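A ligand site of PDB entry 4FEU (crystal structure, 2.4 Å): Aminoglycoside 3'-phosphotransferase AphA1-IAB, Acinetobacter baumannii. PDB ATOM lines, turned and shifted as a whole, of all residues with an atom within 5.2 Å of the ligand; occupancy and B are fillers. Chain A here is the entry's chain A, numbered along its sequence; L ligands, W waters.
OE1 of Glu 270 is in salt-bridge range of N3 of the ligand, at 2.5 Å.
The side-chain carboxylate (OE2) of Glu 239 lies within hydrogen-bond range of an oxygen (O10) of the ligand, 2.6 Å away.
The backbone carbonyl oxygen (O) of Asp 269 is in hydrogen-bond range of a nitrogen (N2) of the ligand, at 2.7 Å.
The side-chain carboxylate (OD2) of Asp 269 is in salt-bridge range of a nitrogen (N2) of the ligand (3.7 Å).
OD1 of Asp 168 lies within salt-bridge range of N3 of the ligand, 2.8 Å away.
O3 of the ligand lies within hydrogen-bond range of OD2 of Asp 199, 2.7 Å away.
A nitrogen (N2) of the ligand is in salt-bridge range of the chain-end carboxylate (O) of Phe 272, at 2.8 Å.
The backbone carbonyl oxygen (O) of Asp 166 lies within hydrogen-bond range of a nitrogen (N3) of the ligand, at 3.0 Å.
O4 of the ligand lies within hydrogen-bond range of NH1 of Arg 220 (3.4 Å).
OE2 of Glu 270 is in hydrogen-bond range of N of Asp 168.
The side-chain carboxylate (OD1) of Asp 269 lies within salt-bridge range of the guanidinium group (NH2) of Arg 220 (3.6 Å).
The side-chain carboxylate (OD1) of Asp 168 is in hydrogen-bond range of the side-chain amide nitrogen (ND2) of Asn 235 (3.2 Å).
OD2 of Asp 199 lies within salt-bridge range of NH2 of Arg 220, 3.8 Å away.
The side-chain amide nitrogen (ND2) of Asn 204 lies within hydrogen-bond range of the backbone carbonyl oxygen (O) of Asp 199, 2.8 Å away.
The chain-end carboxylate of Phe 272 is in salt-bridge range of the guanidinium group of Arg 220, at 3.9 Å.
OXT of Phe 272 lies within salt-bridge range of NH1 of Arg 156 (3.4 Å).
Residues that only touch the ligand: Asn 235, Cys 236, Phe 167, Asp 217 and Gly 35.
Within 4 Å of the ligand: Gly 35, Asp 166, Phe 167, Asp 168, Asp 199, Asp 217, Arg 220, Asn 235, Cys 236, Glu 239, Asp 269, Glu 270 and Phe 272.
Along chain A the residues within 4 Å of the ligand span positions 35 to 272.
Water W1 bridges an oxygen (O4) of the ligand (2.7 Å) and the backbone NH (N) of Ser 37 (3.3 Å).
Water W9 lies within hydrogen-bond range of the side-chain carboxylate of Asp 199 (2.7 Å), an oxygen (O2) of the ligand (2.8 Å) and the side-chain carboxylate of Asp 269 (3.2 Å).
Water W6 bridges an oxygen (O11) of the ligand and the side-chain sulfur of Cys 236.
Water W8 lies within hydrogen-bond range of OD2 of Asp 168 and N3 of the ligand.
Water W5 lies within hydrogen-bond range of O3 of the ligand (3.2 Å) and OD2 of Asp 203 (3.4 Å).
Water W4 lies within hydrogen-bond range of N of Asp 169 (2.7 Å) and N4 of the ligand (3.4 Å).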
ATOM      1  N   GLY A  35      -2.285 -11.910 -15.063  1.00  0.00           N
ATOM      2  CA  GLY A  35      -1.355 -11.140 -15.894  1.00  0.00           C
ATOM      3  C   GLY A  35      -0.343 -11.988 -16.639  1.00  0.00           C
ATOM      4  O   GLY A  35       0.780 -11.546 -16.876  1.00  0.00           O
ATOM      5  N   GLN A  36      -0.760 -13.220 -17.022  1.00  0.00           N
ATOM      6  CA  GLN A  36       0.079 -14.194 -17.739  1.00  0.00           C
ATOM      7  C   GLN A  36       0.194 -13.863 -19.230  1.00  0.00           C
ATOM      8  O   GLN A  36      -0.472 -12.960 -19.728  1.00  0.00           O
ATOM      9  CB  GLN A  36      -0.404 -15.652 -17.496  1.00  0.00           C
ATOM     10  CG  GLN A  36      -1.749 -16.044 -18.146  1.00  0.00           C
ATOM     11  CD  GLN A  36      -2.986 -15.535 -17.421  1.00  0.00           C
ATOM     12  OE1 GLN A  36      -2.937 -15.144 -16.244  1.00  0.00           O
ATOM     13  NE2 GLN A  36      -4.128 -15.537 -18.097  1.00  0.00           N
ATOM     14  N   SER A  37       1.067 -14.612 -19.930  1.00  0.00           N
ATOM     15  CA  SER A  37       1.288 -14.424 -21.352  1.00  0.00           C
ATOM     16  C   SER A  37       0.812 -15.635 -22.172  1.00  0.00           C
ATOM     17  O   SER A  37       1.475 -16.682 -22.232  1.00  0.00           O
ATOM     18  CB  SER A  37       2.742 -14.045 -21.653  1.00  0.00           C
ATOM     19  OG  SER A  37       3.674 -14.958 -21.096  1.00  0.00           O
ATOM     20  N   ARG A 156      11.041 -12.079 -29.577  1.00  0.00           N
ATOM     21  CA  ARG A 156       9.949 -11.306 -28.997  1.00  0.00           C
ATOM     22  C   ARG A 156      10.088  -9.812 -29.354  1.00  0.00           C
ATOM     23  O   ARG A 156       9.090  -9.164 -29.603  1.00  0.00           O
ATOM     24  CB  ARG A 156       9.893 -11.521 -27.476  1.00  0.00           C
ATOM     25  CG  ARG A 156       9.567 -12.956 -27.050  1.00  0.00           C
ATOM     26  CD  ARG A 156       8.196 -13.106 -26.408  1.00  0.00           C
ATOM     27  NE  ARG A 156       8.010 -12.217 -25.262  1.00  0.00           N
ATOM     28  CZ  ARG A 156       6.832 -11.734 -24.874  1.00  0.00           C
ATOM     29  NH1 ARG A 156       6.768 -10.905 -23.838  1.00  0.00           N
ATOM     30  NH2 ARG A 156       5.727 -12.075 -25.503  1.00  0.00           N
ATOM     31  N   ASP A 163       6.398  -5.795 -24.175  1.00  0.00           N
ATOM     32  CA  ASP A 163       5.658  -4.582 -23.823  1.00  0.00           C
ATOM     33  C   ASP A 163       6.496  -3.582 -23.041  1.00  0.00           C
ATOM     34  O   ASP A 163       6.783  -3.800 -21.863  1.00  0.00           O
ATOM     35  CB  ASP A 163       4.243  -4.837 -23.262  1.00  0.00           C
ATOM     36  CG  ASP A 163       4.163  -5.747 -22.070  1.00  0.00           C
ATOM     37  OD1 ASP A 163       4.791  -6.839 -22.106  1.00  0.00           O
ATOM     38  OD2 ASP A 163       3.382  -5.434 -21.140  1.00  0.00           O
ATOM     39  N   ASP A 166       5.326  -2.296 -19.349  1.00  0.00           N
ATOM     40  CA  ASP A 166       5.594  -3.052 -18.113  1.00  0.00           C
ATOM     41  C   ASP A 166       7.071  -3.058 -17.698  1.00  0.00           C
ATOM     42  O   ASP A 166       7.457  -3.876 -16.855  1.00  0.00           O
ATOM     43  CB  ASP A 166       5.040  -4.487 -18.246  1.00  0.00           C
ATOM     44  CG  ASP A 166       4.652  -5.154 -16.938  1.00  0.00           C
ATOM     45  OD1 ASP A 166       4.435  -4.428 -15.946  1.00  0.00           O
ATOM     46  OD2 ASP A 166       4.543  -6.402 -16.918  1.00  0.00           O
ATOM     47  N   PHE A 167       7.901  -2.145 -18.255  1.00  0.00           N
ATOM     48  CA  PHE A 167       9.320  -2.042 -17.904  1.00  0.00           C
ATOM     49  C   PHE A 167       9.484  -1.527 -16.476  1.00  0.00           C
ATOM     50  O   PHE A 167       8.582  -0.845 -15.951  1.00  0.00           O
ATOM     51  CB  PHE A 167      10.072  -1.091 -18.870  1.00  0.00           C
ATOM     52  CG  PHE A 167      10.428  -1.574 -20.257  1.00  0.00           C
ATOM     53  CD1 PHE A 167      10.242  -2.911 -20.612  1.00  0.00           C
ATOM     54  CD2 PHE A 167      10.981  -0.715 -21.189  1.00  0.00           C
ATOM     55  CE1 PHE A 167      10.567  -3.344 -21.915  1.00  0.00           C
ATOM     56  CE2 PHE A 167      11.322  -1.160 -22.469  1.00  0.00           C
ATOM     57  CZ  PHE A 167      11.115  -2.473 -22.827  1.00  0.00           C
ATOM     58  N   ASP A 168      10.642  -1.821 -15.848  1.00  0.00           N
ATOM     59  CA  ASP A 168      10.980  -1.310 -14.525  1.00  0.00           C
ATOM     60  C   ASP A 168      11.198   0.214 -14.642  1.00  0.00           C
ATOM     61  O   ASP A 168      11.492   0.704 -15.722  1.00  0.00           O
ATOM     62  CB  ASP A 168      12.238  -2.019 -13.980  1.00  0.00           C
ATOM     63  CG  ASP A 168      12.087  -3.518 -13.804  1.00  0.00           C
ATOM     64  OD1 ASP A 168      10.982  -3.970 -13.434  1.00  0.00           O
ATOM     65  OD2 ASP A 168      13.110  -4.240 -13.989  1.00  0.00           O
ATOM     66  N   ASP A 169      10.956   0.953 -13.541  1.00  0.00           N
ATOM     67  CA  ASP A 169      11.048   2.419 -13.514  1.00  0.00           C
ATOM     68  C   ASP A 169      12.302   3.022 -14.157  1.00  0.00           C
ATOM     69  O   ASP A 169      12.168   3.942 -14.954  1.00  0.00           O
ATOM     70  CB  ASP A 169      10.803   2.975 -12.102  1.00  0.00           C
ATOM     71  CG  ASP A 169       9.434   2.691 -11.496  1.00  0.00           C
ATOM     72  OD1 ASP A 169       8.600   2.044 -12.175  1.00  0.00           O
ATOM     73  OD2 ASP A 169       9.182   3.124 -10.353  1.00  0.00           O
ATOM     74  N   ASP A 199      10.913 -17.739 -13.177  1.00  0.00           N
ATOM     75  CA  ASP A 199       9.973 -16.669 -12.856  1.00  0.00           C
ATOM     76  C   ASP A 199       9.714 -16.740 -11.326  1.00  0.00           C
ATOM     77  O   ASP A 199       8.587 -16.961 -10.872  1.00  0.00           O
ATOM     78  CB  ASP A 199       8.667 -16.804 -13.694  1.00  0.00           C
ATOM     79  CG  ASP A 199       7.800 -15.543 -13.863  1.00  0.00           C
ATOM     80  OD1 ASP A 199       8.204 -14.455 -13.355  1.00  0.00           O
ATOM     81  OD2 ASP A 199       6.757 -15.622 -14.539  1.00  0.00           O
ATOM     82  N   SER A 201       8.932 -15.035  -8.815  1.00  0.00           N
ATOM     83  CA  SER A 201       8.257 -13.818  -8.391  1.00  0.00           C
ATOM     84  C   SER A 201       7.366 -14.076  -7.171  1.00  0.00           C
ATOM     85  O   SER A 201       7.095 -15.237  -6.843  1.00  0.00           O
ATOM     86  CB  SER A 201       7.462 -13.225  -9.554  1.00  0.00           C
ATOM     87  OG  SER A 201       6.257 -13.927  -9.825  1.00  0.00           O
ATOM     88  N   ASP A 203       4.248 -13.768  -6.961  1.00  0.00           N
ATOM     89  CA  ASP A 203       2.964 -14.368  -7.376  1.00  0.00           C
ATOM     90  C   ASP A 203       3.072 -15.878  -7.573  1.00  0.00           C
ATOM     91  O   ASP A 203       2.065 -16.576  -7.607  1.00  0.00           O
ATOM     92  CB  ASP A 203       2.427 -13.723  -8.667  1.00  0.00           C
ATOM     93  CG  ASP A 203       2.326 -12.211  -8.651  1.00  0.00           C
ATOM     94  OD1 ASP A 203       1.861 -11.665  -7.637  1.00  0.00           O
ATOM     95  OD2 ASP A 203       2.719 -11.593  -9.652  1.00  0.00           O
ATOM     96  N   ASN A 204       4.303 -16.372  -7.696  1.00  0.00           N
ATOM     97  CA  ASN A 204       4.571 -17.777  -7.961  1.00  0.00           C
ATOM     98  C   ASN A 204       4.915 -18.636  -6.762  1.00  0.00           C
ATOM     99  O   ASN A 204       5.016 -19.847  -6.911  1.00  0.00           O
ATOM    100  CB  ASN A 204       5.570 -17.922  -9.094  1.00  0.00           C
ATOM    101  CG  ASN A 204       4.982 -17.385 -10.375  1.00  0.00           C
ATOM    102  OD1 ASN A 204       3.771 -17.356 -10.544  1.00  0.00           O
ATOM    103  ND2 ASN A 204       5.825 -16.924 -11.276  1.00  0.00           N
ATOM    104  N   ASP A 217       3.922 -21.998 -11.923  1.00  0.00           N
ATOM    105  CA  ASP A 217       4.415 -21.341 -13.137  1.00  0.00           C
ATOM    106  C   ASP A 217       5.840 -21.765 -13.463  1.00  0.00           C
ATOM    107  O   ASP A 217       6.757 -20.937 -13.586  1.00  0.00           O
ATOM    108  CB  ASP A 217       4.248 -19.798 -13.005  1.00  0.00           C
ATOM    109  CG  ASP A 217       4.208 -19.019 -14.307  1.00  0.00           C
ATOM    110  OD1 ASP A 217       4.348 -19.645 -15.383  1.00  0.00           O
ATOM    111  OD2 ASP A 217       4.068 -17.769 -14.244  1.00  0.00           O
ATOM    112  N   ARG A 220       9.496 -22.181 -17.329  1.00  0.00           N
ATOM    113  CA  ARG A 220      10.880 -21.743 -17.629  1.00  0.00           C
ATOM    114  C   ARG A 220      11.953 -22.494 -16.864  1.00  0.00           C
ATOM    115  O   ARG A 220      13.134 -22.131 -16.960  1.00  0.00           O
ATOM    116  CB  ARG A 220      11.059 -20.215 -17.395  1.00  0.00           C
ATOM    117  CG  ARG A 220      10.186 -19.301 -18.242  1.00  0.00           C
ATOM    118  CD  ARG A 220      10.553 -17.835 -18.097  1.00  0.00           C
ATOM    119  NE  ARG A 220       9.477 -16.964 -18.583  1.00  0.00           N
ATOM    120  CZ  ARG A 220       9.082 -15.836 -17.991  1.00  0.00           C
ATOM    121  NH1 ARG A 220       8.087 -15.130 -18.498  1.00  0.00           N
ATOM    122  NH2 ARG A 220       9.697 -15.398 -16.894  1.00  0.00           N
ATOM    123  N   ASN A 235      13.743  -7.767  -7.204  1.00  0.00           N
ATOM    124  CA  ASN A 235      12.983  -6.701  -7.833  1.00  0.00           C
ATOM    125  C   ASN A 235      11.578  -6.621  -7.247  1.00  0.00           C
ATOM    126  O   ASN A 235      11.148  -5.546  -6.882  1.00  0.00           O
ATOM    127  CB  ASN A 235      12.947  -6.905  -9.321  1.00  0.00           C
ATOM    128  CG  ASN A 235      12.492  -5.691 -10.078  1.00  0.00           C
ATOM    129  OD1 ASN A 235      12.989  -4.580  -9.891  1.00  0.00           O
ATOM    130  ND2 ASN A 235      11.548  -5.885 -10.969  1.00  0.00           N
ATOM    131  N   CYS A 236      10.885  -7.768  -7.124  1.00  0.00           N
ATOM    132  CA  CYS A 236       9.555  -7.838  -6.510  1.00  0.00           C
ATOM    133  C   CYS A 236       9.618  -7.216  -5.106  1.00  0.00           C
ATOM    134  O   CYS A 236       8.805  -6.367  -4.788  1.00  0.00           O
ATOM    135  CB  CYS A 236       9.062  -9.279  -6.450  1.00  0.00           C
ATOM    136  SG  CYS A 236       8.610  -9.992  -8.047  1.00  0.00           S
ATOM    137  N   GLU A 239       9.364  -3.292  -4.146  1.00  0.00           N
ATOM    138  CA  GLU A 239       8.116  -2.576  -3.936  1.00  0.00           C
ATOM    139  C   GLU A 239       7.600  -2.635  -2.486  1.00  0.00           C
ATOM    140  O   GLU A 239       6.560  -2.070  -2.183  1.00  0.00           O
ATOM    141  CB  GLU A 239       7.065  -2.884  -5.030  1.00  0.00           C
ATOM    142  CG  GLU A 239       6.432  -4.254  -4.981  1.00  0.00           C
ATOM    143  CD  GLU A 239       5.857  -4.694  -6.319  1.00  0.00           C
ATOM    144  OE1 GLU A 239       4.804  -4.153  -6.718  1.00  0.00           O
ATOM    145  OE2 GLU A 239       6.444  -5.610  -6.938  1.00  0.00           O
ATOM    146  N   ASP A 269      14.399 -10.010 -18.264  1.00  0.00           N
ATOM    147  CA  ASP A 269      12.997 -10.252 -17.915  1.00  0.00           C
ATOM    148  C   ASP A 269      12.020  -9.236 -18.545  1.00  0.00           C
ATOM    149  O   ASP A 269      10.826  -9.524 -18.598  1.00  0.00           O
ATOM    150  CB  ASP A 269      12.771 -10.375 -16.389  1.00  0.00           C
ATOM    151  CG  ASP A 269      11.497 -11.119 -16.024  1.00  0.00           C
ATOM    152  OD1 ASP A 269      11.276 -12.229 -16.555  1.00  0.00           O
ATOM    153  OD2 ASP A 269      10.743 -10.618 -15.173  1.00  0.00           O
ATOM    154  N   GLU A 270      12.530  -8.109 -19.094  1.00  0.00           N
ATOM    155  CA  GLU A 270      11.711  -7.084 -19.761  1.00  0.00           C
ATOM    156  C   GLU A 270      11.091  -7.571 -21.064  1.00  0.00           C
ATOM    157  O   GLU A 270      10.055  -7.071 -21.499  1.00  0.00           O
ATOM    158  CB  GLU A 270      12.517  -5.800 -20.066  1.00  0.00           C
ATOM    159  CG  GLU A 270      13.169  -5.138 -18.871  1.00  0.00           C
ATOM    160  CD  GLU A 270      12.249  -4.421 -17.908  1.00  0.00           C
ATOM    161  OE1 GLU A 270      11.100  -4.880 -17.720  1.00  0.00           O
ATOM    162  OE2 GLU A 270      12.686  -3.408 -17.320  1.00  0.00           O
ATOM    163  N   PHE A 272       9.957 -10.569 -21.660  1.00  0.00           N
ATOM    164  CA  PHE A 272       9.037 -11.688 -21.405  1.00  0.00           C
ATOM    165  C   PHE A 272       7.713 -11.309 -20.719  1.00  0.00           C
ATOM    166  O   PHE A 272       7.566 -10.155 -20.243  1.00  0.00           O
ATOM    167  CB  PHE A 272       9.765 -12.829 -20.649  1.00  0.00           C
ATOM    168  CG  PHE A 272      10.971 -13.342 -21.394  1.00  0.00           C
ATOM    169  CD1 PHE A 272      10.852 -14.350 -22.346  1.00  0.00           C
ATOM    170  CD2 PHE A 272      12.238 -12.784 -21.177  1.00  0.00           C
ATOM    171  CE1 PHE A 272      11.970 -14.807 -23.040  1.00  0.00           C
ATOM    172  CE2 PHE A 272      13.348 -13.226 -21.893  1.00  0.00           C
ATOM    173  CZ  PHE A 272      13.206 -14.230 -22.825  1.00  0.00           C
ATOM    174  OXT PHE A 272       6.789 -12.152 -20.705  1.00  0.00           O
HETATM  175  C1  LIG L   1       5.236 -10.178 -15.276  1.00  0.00           C
HETATM  176  C2  LIG L   1       4.866 -11.496 -14.532  1.00  0.00           C
HETATM  177  C3  LIG L   1       5.164 -12.741 -15.396  1.00  0.00           C
HETATM  178  C4  LIG L   1       4.588 -12.618 -16.794  1.00  0.00           C
HETATM  179  C5  LIG L   1       4.970 -11.272 -17.430  1.00  0.00           C
HETATM  180  C6  LIG L   1       4.254 -11.127 -18.784  1.00  0.00           C
HETATM  181  C7  LIG L   1       9.092  -6.529 -15.427  1.00  0.00           C
HETATM  182  C8  LIG L   1       7.769  -6.329 -14.691  1.00  0.00           C
HETATM  183  C9  LIG L   1       7.203  -7.744 -14.425  1.00  0.00           C
HETATM  184  C10 LIG L   1       7.055  -8.596 -15.706  1.00  0.00           C
HETATM  185  C11 LIG L   1       8.399  -8.590 -16.453  1.00  0.00           C
HETATM  186  C12 LIG L   1       8.819  -7.167 -16.765  1.00  0.00           C
HETATM  187  C13 LIG L   1       7.052  -4.931 -12.870  1.00  0.00           C
HETATM  188  C14 LIG L   1       7.651  -3.732 -12.136  1.00  0.00           C
HETATM  189  C15 LIG L   1       8.434  -4.191 -10.907  1.00  0.00           C
HETATM  190  C16 LIG L   1       7.545  -5.079 -10.012  1.00  0.00           C
HETATM  191  C17 LIG L   1       7.006  -6.270 -10.816  1.00  0.00           C
HETATM  192  C18 LIG L   1       6.131  -7.136  -9.882  1.00  0.00           C
HETATM  193  N1  LIG L   1       4.855  -9.992 -19.503  1.00  0.00           N
HETATM  194  N2  LIG L   1       8.331  -9.350 -17.712  1.00  0.00           N
HETATM  195  N3  LIG L   1       9.825  -5.271 -15.592  1.00  0.00           N
HETATM  196  N4  LIG L   1       8.896  -3.025 -10.134  1.00  0.00           N
HETATM  197  O1  LIG L   1       4.647 -10.150 -16.594  1.00  0.00           O
HETATM  198  O2  LIG L   1       5.603 -11.568 -13.296  1.00  0.00           O
HETATM  199  O3  LIG L   1       4.627 -13.930 -14.811  1.00  0.00           O
HETATM  200  O4  LIG L   1       5.113 -13.702 -17.578  1.00  0.00           O
HETATM  201  O5  LIG L   1       6.661  -9.955 -15.411  1.00  0.00           O
HETATM  202  O6  LIG L   1       5.935  -7.650 -13.757  1.00  0.00           O
HETATM  203  O7  LIG L   1       8.141  -5.673 -13.463  1.00  0.00           O
HETATM  204  O8  LIG L   1       6.282  -5.766 -11.967  1.00  0.00           O
HETATM  205  O9  LIG L   1       8.509  -3.000 -13.025  1.00  0.00           O
HETATM  206  O10 LIG L   1       8.259  -5.533  -8.867  1.00  0.00           O
HETATM  207  O11 LIG L   1       5.923  -8.432 -10.454  1.00  0.00           O
HETATM  208  O   HOH W   1       3.338 -15.721 -17.845  1.00  0.00           O
HETATM  209  O   HOH W   2       5.213 -10.997  -8.579  1.00  0.00           O
HETATM  210  O   HOH W   3       6.552  -1.473 -14.291  1.00  0.00           O
HETATM  211  O   HOH W   4      10.776  -0.363 -11.181  1.00  0.00           O
HETATM  212  O   HOH W   5       2.966 -13.928 -12.132  1.00  0.00           O
HETATM  213  O   HOH W   6       8.452  -9.757 -11.377  1.00  0.00           O
HETATM  214  O   HOH W   7       8.309 -12.386 -17.206  1.00  0.00           O
HETATM  215  O   HOH W   8      12.456  -6.820 -14.818  1.00  0.00           O
HETATM  216  O   HOH W   9       8.374 -11.746 -13.369  1.00  0.00           O
